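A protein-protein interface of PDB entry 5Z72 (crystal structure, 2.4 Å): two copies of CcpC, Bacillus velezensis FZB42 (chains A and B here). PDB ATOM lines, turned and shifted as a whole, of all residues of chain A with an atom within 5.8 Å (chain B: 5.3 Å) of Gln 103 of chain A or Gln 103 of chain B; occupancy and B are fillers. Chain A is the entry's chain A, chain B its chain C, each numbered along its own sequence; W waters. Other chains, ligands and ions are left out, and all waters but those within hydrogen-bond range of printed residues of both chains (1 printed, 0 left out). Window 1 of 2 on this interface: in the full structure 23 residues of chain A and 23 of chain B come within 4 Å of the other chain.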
ATOM      1  N   ALA A  98      -1.469 -21.290  26.407  1.00  0.00           N
ATOM      2  CA  ALA A  98      -1.838 -22.003  25.235  1.00  0.00           C
ATOM      3  C   ALA A  98      -3.247 -21.564  24.875  1.00  0.00           C
ATOM      4  O   ALA A  98      -4.085 -21.390  25.779  1.00  0.00           O
ATOM      5  CB  ALA A  98      -1.764 -23.532  25.464  1.00  0.00           C
ATOM      6  N   SER A  99      -3.510 -21.424  23.574  1.00  0.00           N
ATOM      7  CA  SER A  99      -4.736 -20.729  23.073  1.00  0.00           C
ATOM      8  C   SER A  99      -6.029 -21.257  23.546  1.00  0.00           C
ATOM      9  O   SER A  99      -6.835 -20.471  24.027  1.00  0.00           O
ATOM     10  CB  SER A  99      -4.794 -20.759  21.559  1.00  0.00           C
ATOM     11  OG  SER A  99      -3.746 -19.951  21.076  1.00  0.00           O
ATOM     12  N   ILE A 100      -6.231 -22.581  23.412  1.00  0.00           N
ATOM     13  CA  ILE A 100      -7.505 -23.176  23.803  1.00  0.00           C
ATOM     14  C   ILE A 100      -7.694 -23.092  25.303  1.00  0.00           C
ATOM     15  O   ILE A 100      -8.814 -23.048  25.772  1.00  0.00           O
ATOM     16  CB  ILE A 100      -7.665 -24.675  23.392  1.00  0.00           C
ATOM     17  CG1 ILE A 100      -6.583 -25.556  24.049  1.00  0.00           C
ATOM     18  CG2 ILE A 100      -7.632 -24.809  21.931  1.00  0.00           C
ATOM     19  CD1 ILE A 100      -6.605 -27.030  23.638  1.00  0.00           C
ATOM     20  N   ILE A 101      -6.610 -23.076  26.062  1.00  0.00           N
ATOM     21  CA  ILE A 101      -6.735 -22.898  27.486  1.00  0.00           C
ATOM     22  C   ILE A 101      -7.204 -21.491  27.747  1.00  0.00           C
ATOM     23  O   ILE A 101      -8.118 -21.254  28.599  1.00  0.00           O
ATOM     24  CB  ILE A 101      -5.398 -23.127  28.252  1.00  0.00           C
ATOM     25  CG1 ILE A 101      -4.940 -24.576  28.094  1.00  0.00           C
ATOM     26  CG2 ILE A 101      -5.580 -22.759  29.705  1.00  0.00           C
ATOM     27  CD1 ILE A 101      -5.979 -25.571  28.483  1.00  0.00           C
ATOM     28  N   GLY A 102      -6.559 -20.563  27.040  1.00  0.00           N
ATOM     29  CA  GLY A 102      -6.877 -19.144  27.162  1.00  0.00           C
ATOM     30  C   GLY A 102      -8.348 -18.901  26.920  1.00  0.00           C
ATOM     31  O   GLY A 102      -9.009 -18.155  27.647  1.00  0.00           O
ATOM     32  N   GLN A 103      -8.860 -19.566  25.905  1.00  0.00           N
ATOM     33  CA  GLN A 103     -10.249 -19.429  25.551  1.00  0.00           C
ATOM     34  C   GLN A 103     -11.216 -20.147  26.425  1.00  0.00           C
ATOM     35  O   GLN A 103     -12.237 -19.580  26.781  1.00  0.00           O
ATOM     36  CB  GLN A 103     -10.448 -19.920  24.146  1.00  0.00           C
ATOM     37  CG  GLN A 103      -9.927 -18.899  23.112  1.00  0.00           C
ATOM     38  CD  GLN A 103     -10.772 -18.884  21.846  1.00  0.00           C
ATOM     39  OE1 GLN A 103     -12.025 -18.922  21.903  1.00  0.00           O
ATOM     40  NE2 GLN A 103     -10.101 -18.836  20.693  1.00  0.00           N
ATOM     41  N   HIS A 104     -10.940 -21.413  26.716  1.00  0.00           N
ATOM     42  CA  HIS A 104     -11.972 -22.269  27.266  1.00  0.00           C
ATOM     43  C   HIS A 104     -11.897 -22.524  28.799  1.00  0.00           C
ATOM     44  O   HIS A 104     -12.906 -22.797  29.430  1.00  0.00           O
ATOM     45  CB  HIS A 104     -11.946 -23.584  26.515  1.00  0.00           C
ATOM     46  CG  HIS A 104     -12.421 -23.473  25.103  1.00  0.00           C
ATOM     47  ND1 HIS A 104     -13.756 -23.408  24.777  1.00  0.00           N
ATOM     48  CD2 HIS A 104     -11.745 -23.406  23.928  1.00  0.00           C
ATOM     49  CE1 HIS A 104     -13.882 -23.310  23.465  1.00  0.00           C
ATOM     50  NE2 HIS A 104     -12.676 -23.307  22.927  1.00  0.00           N
ATOM     51  N   TRP A 105     -10.736 -22.383  29.405  1.00  0.00           N
ATOM     52  CA  TRP A 105     -10.575 -22.771  30.790  1.00  0.00           C
ATOM     53  C   TRP A 105     -10.197 -21.591  31.640  1.00  0.00           C
ATOM     54  O   TRP A 105     -10.629 -21.499  32.782  1.00  0.00           O
ATOM     55  CB  TRP A 105      -9.504 -23.856  30.890  1.00  0.00           C
ATOM     56  CG  TRP A 105      -9.309 -24.375  32.227  1.00  0.00           C
ATOM     57  CD1 TRP A 105     -10.091 -25.284  32.855  1.00  0.00           C
ATOM     58  CD2 TRP A 105      -8.265 -24.036  33.144  1.00  0.00           C
ATOM     59  NE1 TRP A 105      -9.604 -25.543  34.106  1.00  0.00           N
ATOM     60  CE2 TRP A 105      -8.474 -24.792  34.309  1.00  0.00           C
ATOM     61  CE3 TRP A 105      -7.175 -23.170  33.098  1.00  0.00           C
ATOM     62  CZ2 TRP A 105      -7.626 -24.722  35.413  1.00  0.00           C
ATOM     63  CZ3 TRP A 105      -6.332 -23.107  34.198  1.00  0.00           C
ATOM     64  CH2 TRP A 105      -6.573 -23.876  35.335  1.00  0.00           C
ATOM     65  N   LEU A 106      -9.408 -20.672  31.073  1.00  0.00           N
ATOM     66  CA  LEU A 106      -8.834 -19.559  31.839  1.00  0.00           C
ATOM     67  C   LEU A 106      -9.828 -18.452  32.327  1.00  0.00           C
ATOM     68  O   LEU A 106      -9.693 -17.945  33.448  1.00  0.00           O
ATOM     69  CB  LEU A 106      -7.711 -18.916  31.012  1.00  0.00           C
ATOM     70  CG  LEU A 106      -6.934 -17.833  31.757  1.00  0.00           C
ATOM     71  CD1 LEU A 106      -6.185 -18.372  32.976  1.00  0.00           C
ATOM     72  CD2 LEU A 106      -5.999 -17.160  30.814  1.00  0.00           C
ATOM     73  N   PRO A 107     -10.822 -18.086  31.513  1.00  0.00           N
ATOM     74  CA  PRO A 107     -11.866 -17.156  31.971  1.00  0.00           C
ATOM     75  C   PRO A 107     -12.438 -17.454  33.353  1.00  0.00           C
ATOM     76  O   PRO A 107     -12.506 -16.528  34.145  1.00  0.00           O
ATOM     77  CB  PRO A 107     -12.939 -17.318  30.914  1.00  0.00           C
ATOM     78  CG  PRO A 107     -12.164 -17.564  29.659  1.00  0.00           C
ATOM     79  CD  PRO A 107     -11.046 -18.491  30.119  1.00  0.00           C
ATOM     80  N   GLU A 219      -9.563 -23.624  17.492  1.00  0.00           N
ATOM     81  CA  GLU A 219     -10.903 -23.024  17.522  1.00  0.00           C
ATOM     82  C   GLU A 219     -11.506 -22.856  16.108  1.00  0.00           C
ATOM     83  O   GLU A 219     -12.704 -23.000  15.906  1.00  0.00           O
ATOM     84  CB  GLU A 219     -10.863 -21.665  18.225  1.00  0.00           C
ATOM     85  CG  GLU A 219     -12.236 -21.063  18.400  1.00  0.00           C
ATOM     86  CD  GLU A 219     -13.124 -21.868  19.359  1.00  0.00           C
ATOM     87  OE1 GLU A 219     -12.591 -22.468  20.349  1.00  0.00           O
ATOM     88  OE2 GLU A 219     -14.364 -21.877  19.114  1.00  0.00           O
ATOM     89  N   THR A 220     -10.657 -22.580  15.130  1.00  0.00           N
ATOM     90  CA  THR A 220     -11.106 -22.478  13.775  1.00  0.00           C
ATOM     91  C   THR A 220     -11.537 -23.848  13.233  1.00  0.00           C
ATOM     92  O   THR A 220     -12.529 -23.921  12.500  1.00  0.00           O
ATOM     93  CB  THR A 220     -10.016 -21.828  12.912  1.00  0.00           C
ATOM     94  OG1 THR A 220      -9.998 -20.415  13.206  1.00  0.00           O
ATOM     95  CG2 THR A 220     -10.303 -22.025  11.422  1.00  0.00           C
ATOM     96  N   GLN A 223     -14.976 -24.299  14.810  1.00  0.00           N
ATOM     97  CA  GLN A 223     -15.959 -23.466  14.097  1.00  0.00           C
ATOM     98  C   GLN A 223     -16.278 -24.015  12.701  1.00  0.00           C
ATOM     99  O   GLN A 223     -17.434 -24.193  12.331  1.00  0.00           O
ATOM    100  CB  GLN A 223     -15.424 -22.045  14.034  1.00  0.00           C
ATOM    101  CG  GLN A 223     -16.331 -21.034  14.555  1.00  0.00           C
ATOM    102  CD  GLN A 223     -17.083 -21.464  15.746  1.00  0.00           C
ATOM    103  OE1 GLN A 223     -18.316 -21.431  15.747  1.00  0.00           O
ATOM    104  NE2 GLN A 223     -16.357 -21.897  16.795  1.00  0.00           N
ATOM    105  N   ALA B  98      -6.955 -12.435   9.039  1.00  0.00           N
ATOM    106  CA  ALA B  98      -6.898 -11.862  10.380  1.00  0.00           C
ATOM    107  C   ALA B  98      -7.686 -12.757  11.349  1.00  0.00           C
ATOM    108  O   ALA B  98      -8.686 -13.354  10.947  1.00  0.00           O
ATOM    109  CB  ALA B  98      -7.449 -10.472  10.386  1.00  0.00           C
ATOM    110  N   SER B  99      -7.281 -12.844  12.616  1.00  0.00           N
ATOM    111  CA  SER B  99      -7.869 -13.888  13.512  1.00  0.00           C
ATOM    112  C   SER B  99      -9.396 -13.848  13.625  1.00  0.00           C
ATOM    113  O   SER B  99     -10.060 -14.869  13.364  1.00  0.00           O
ATOM    114  CB  SER B  99      -7.273 -13.804  14.921  1.00  0.00           C
ATOM    115  OG  SER B  99      -5.864 -13.948  14.864  1.00  0.00           O
ATOM    116  N   ILE B 100      -9.967 -12.701  14.003  1.00  0.00           N
ATOM    117  CA  ILE B 100     -11.429 -12.609  14.117  1.00  0.00           C
ATOM    118  C   ILE B 100     -12.127 -12.895  12.789  1.00  0.00           C
ATOM    119  O   ILE B 100     -13.201 -13.476  12.741  1.00  0.00           O
ATOM    120  CB  ILE B 100     -11.895 -11.223  14.641  1.00  0.00           C
ATOM    121  CG1 ILE B 100     -11.270 -10.073  13.856  1.00  0.00           C
ATOM    122  CG2 ILE B 100     -11.520 -11.032  16.076  1.00  0.00           C
ATOM    123  CD1 ILE B 100     -11.961  -8.728  14.108  1.00  0.00           C
ATOM    124  N   ILE B 101     -11.512 -12.529  11.680  1.00  0.00           N
ATOM    125  CA  ILE B 101     -12.114 -12.895  10.421  1.00  0.00           C
ATOM    126  C   ILE B 101     -12.071 -14.423  10.246  1.00  0.00           C
ATOM    127  O   ILE B 101     -13.069 -15.050   9.874  1.00  0.00           O
ATOM    128  CB  ILE B 101     -11.412 -12.210   9.239  1.00  0.00           C
ATOM    129  CG1 ILE B 101     -11.442 -10.677   9.396  1.00  0.00           C
ATOM    130  CG2 ILE B 101     -12.049 -12.676   7.979  1.00  0.00           C
ATOM    131  CD1 ILE B 101     -12.725 -10.105  10.021  1.00  0.00           C
ATOM    132  N   GLY B 102     -10.905 -15.005  10.509  1.00  0.00           N
ATOM    133  CA  GLY B 102     -10.732 -16.435  10.386  1.00  0.00           C
ATOM    134  C   GLY B 102     -11.813 -17.157  11.172  1.00  0.00           C
ATOM    135  O   GLY B 102     -12.394 -18.165  10.719  1.00  0.00           O
ATOM    136  N   GLN B 103     -12.100 -16.620  12.354  1.00  0.00           N
ATOM    137  CA  GLN B 103     -12.980 -17.333  13.269  1.00  0.00           C
ATOM    138  C   GLN B 103     -14.443 -17.153  12.974  1.00  0.00           C
ATOM    139  O   GLN B 103     -15.212 -18.126  13.081  1.00  0.00           O
ATOM    140  CB  GLN B 103     -12.714 -16.904  14.719  1.00  0.00           C
ATOM    141  CG  GLN B 103     -13.204 -17.944  15.757  1.00  0.00           C
ATOM    142  CD  GLN B 103     -12.398 -17.936  17.040  1.00  0.00           C
ATOM    143  OE1 GLN B 103     -12.969 -17.997  18.126  1.00  0.00           O
ATOM    144  NE2 GLN B 103     -11.063 -17.899  16.930  1.00  0.00           N
ATOM    145  N   HIS B 104     -14.830 -15.917  12.625  1.00  0.00           N
ATOM    146  CA  HIS B 104     -16.236 -15.568  12.561  1.00  0.00           C
ATOM    147  C   HIS B 104     -16.823 -15.405  11.150  1.00  0.00           C
ATOM    148  O   HIS B 104     -17.961 -15.820  10.912  1.00  0.00           O
ATOM    149  CB  HIS B 104     -16.466 -14.275  13.344  1.00  0.00           C
ATOM    150  CG  HIS B 104     -16.310 -14.418  14.830  1.00  0.00           C
ATOM    151  ND1 HIS B 104     -17.350 -14.786  15.658  1.00  0.00           N
ATOM    152  CD2 HIS B 104     -15.241 -14.214  15.640  1.00  0.00           C
ATOM    153  CE1 HIS B 104     -16.927 -14.808  16.910  1.00  0.00           C
ATOM    154  NE2 HIS B 104     -15.651 -14.459  16.926  1.00  0.00           N
ATOM    155  N   TRP B 105     -16.086 -14.795  10.221  1.00  0.00           N
ATOM    156  CA  TRP B 105     -16.639 -14.480   8.893  1.00  0.00           C
ATOM    157  C   TRP B 105     -16.317 -15.575   7.907  1.00  0.00           C
ATOM    158  O   TRP B 105     -17.190 -16.029   7.204  1.00  0.00           O
ATOM    159  CB  TRP B 105     -16.099 -13.142   8.378  1.00  0.00           C
ATOM    160  CG  TRP B 105     -16.520 -12.709   6.949  1.00  0.00           C
ATOM    161  CD1 TRP B 105     -17.707 -12.125   6.574  1.00  0.00           C
ATOM    162  CD2 TRP B 105     -15.725 -12.773   5.759  1.00  0.00           C
ATOM    163  NE1 TRP B 105     -17.701 -11.820   5.218  1.00  0.00           N
ATOM    164  CE2 TRP B 105     -16.497 -12.208   4.697  1.00  0.00           C
ATOM    165  CE3 TRP B 105     -14.437 -13.235   5.480  1.00  0.00           C
ATOM    166  CZ2 TRP B 105     -16.027 -12.131   3.396  1.00  0.00           C
ATOM    167  CZ3 TRP B 105     -13.964 -13.144   4.167  1.00  0.00           C
ATOM    168  CH2 TRP B 105     -14.761 -12.591   3.147  1.00  0.00           C
ATOM    169  N   LEU B 106     -15.063 -16.016   7.889  1.00  0.00           N
ATOM    170  CA  LEU B 106     -14.574 -16.994   6.919  1.00  0.00           C
ATOM    171  C   LEU B 106     -15.231 -18.394   6.869  1.00  0.00           C
ATOM    172  O   LEU B 106     -15.244 -19.024   5.823  1.00  0.00           O
ATOM    173  CB  LEU B 106     -13.098 -17.186   7.162  1.00  0.00           C
ATOM    174  CG  LEU B 106     -12.424 -18.044   6.125  1.00  0.00           C
ATOM    175  CD1 LEU B 106     -12.302 -17.262   4.843  1.00  0.00           C
ATOM    176  CD2 LEU B 106     -11.066 -18.438   6.668  1.00  0.00           C
ATOM    177  N   PRO B 107     -15.713 -18.919   7.994  1.00  0.00           N
ATOM    178  CA  PRO B 107     -16.212 -20.281   7.826  1.00  0.00           C
ATOM    179  C   PRO B 107     -17.448 -20.390   6.943  1.00  0.00           C
ATOM    180  O   PRO B 107     -17.601 -21.442   6.315  1.00  0.00           O
ATOM    181  CB  PRO B 107     -16.522 -20.708   9.270  1.00  0.00           C
ATOM    182  CG  PRO B 107     -15.630 -19.954  10.066  1.00  0.00           C
ATOM    183  CD  PRO B 107     -15.430 -18.629   9.410  1.00  0.00           C
ATOM    184  N   GLU B 219     -10.812 -12.587  20.680  1.00  0.00           N
ATOM    185  CA  GLU B 219     -11.785 -13.585  21.126  1.00  0.00           C
ATOM    186  C   GLU B 219     -11.618 -13.879  22.651  1.00  0.00           C
ATOM    187  O   GLU B 219     -12.571 -14.208  23.342  1.00  0.00           O
ATOM    188  CB  GLU B 219     -11.626 -14.851  20.287  1.00  0.00           C
ATOM    189  CG  GLU B 219     -12.459 -16.036  20.740  1.00  0.00           C
ATOM    190  CD  GLU B 219     -13.915 -15.871  20.395  1.00  0.00           C
ATOM    191  OE1 GLU B 219     -14.203 -15.121  19.435  1.00  0.00           O
ATOM    192  OE2 GLU B 219     -14.772 -16.495  21.061  1.00  0.00           O
ATOM    193  N   THR B 220     -10.408 -13.720  23.168  1.00  0.00           N
ATOM    194  CA  THR B 220     -10.195 -13.928  24.565  1.00  0.00           C
ATOM    195  C   THR B 220     -10.890 -12.820  25.316  1.00  0.00           C
ATOM    196  O   THR B 220     -11.564 -13.086  26.324  1.00  0.00           O
ATOM    197  CB  THR B 220      -8.694 -14.005  24.928  1.00  0.00           C
ATOM    198  OG1 THR B 220      -8.147 -15.206  24.382  1.00  0.00           O
ATOM    199  CG2 THR B 220      -8.503 -14.067  26.446  1.00  0.00           C
ATOM    200  N   GLN B 223     -14.586 -13.710  25.336  1.00  0.00           N
ATOM    201  CA  GLN B 223     -14.935 -14.715  26.357  1.00  0.00           C
ATOM    202  C   GLN B 223     -14.875 -14.123  27.770  1.00  0.00           C
ATOM    203  O   GLN B 223     -15.793 -14.292  28.553  1.00  0.00           O
ATOM    204  CB  GLN B 223     -14.041 -15.937  26.263  1.00  0.00           C
ATOM    205  CG  GLN B 223     -14.254 -16.808  25.026  1.00  0.00           C
ATOM    206  CD  GLN B 223     -15.699 -17.175  24.778  1.00  0.00           C
ATOM    207  OE1 GLN B 223     -16.441 -17.451  25.697  1.00  0.00           O
ATOM    208  NE2 GLN B 223     -16.115 -17.124  23.517  1.00  0.00           N
HETATM  209  O   HOH W   1     -18.204 -19.183  13.133  1.00  0.00           O
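Gln 103 of chain A touches just these residues of chain B: Gln 103 (3.9 Å), Glu 219 (3.1 Å) and Gln 223 (3.9 Å). Of the printed residues of chain B, Glu 219 of chain A touches Gln 103. Of the printed residues of chain A, Gln 103 of chain B touches Gln 103, Glu 219 and Gln 223. Trp 105 of chain B touches none of the printed residues of chain A. Of the printed residues of chain A, Gln 223 of chain B touches Gln 103 (3.9 Å). The nearest residue of chain B that does not touch Gln 103 of chain A is Thr 220 of chain B (4.3 Å). The nearest printed residue of chain A that does not touch Gln 103 of chain B is Thr 220 of chain A (4.3 Å).
Of the 13 printed residues of chain A, 3 touch a printed residue of chain B. Among the printed residues, 5 pairs touch across the chains. Among the printed residues, no Asp or Glu carboxylate lies within 4 Å of a Lys or Arg side-chain nitrogen of the other chain.
OE1 of Glu 219 of chain A is in hydrogen-bond range of NE2 of His 104 of chain A (2.7 Å). NE2 of Gln 223 of chain B is in hydrogen-bond range of OE2 of Glu 219 of chain B (2.9 Å). OE1 of Glu 219 of chain B lies close to OE1 of Gln 103 of chain B (3.4 Å). NE2 of Gln 223 of chain A sits at hydrogen-bond distance from OE2 of Glu 219 of chain A (3.1 Å). The side-chain carboxylate of Glu 219 of chain B is in hydrogen-bond range of a ring nitrogen (NE2) of His 104 of chain B (3.0 Å).
Water W1 bridges O of Gln 103 of chain B (3.2 Å) and OE1 of Gln 223 of chain A (3.4 Å).
OE1 of Gln 103 of chain B touches NE2 of Gln 103 of chain A, 3.9 Å away. Glu 219 of chain B touches Gln 103 of chain A. Gln 103 of chain A touches Gln 223 of chain B. CG of Glu 219 of chain A touches OE1 of Gln 103 of chain B, at 3.2 Å. Gln 223 of chain A touches Gln 103 of chain B.
Gln 103 of chain A touches its own counterpart, Gln 103 of chain B. Gln 103 of chain A touches Glu 219 of chain B, and with the chains exchanged Glu 219 of chain A touches Gln 103 of chain B. Gln 103 of chain A touches Gln 223 of chain B, and with the chains exchanged Gln 223 of chain A touches Gln 103 of chain B. Positions printed for both chains: 98, 99, 100, 101, 102, 103, 104, 105, 106, 107, 219, 220 and 223.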
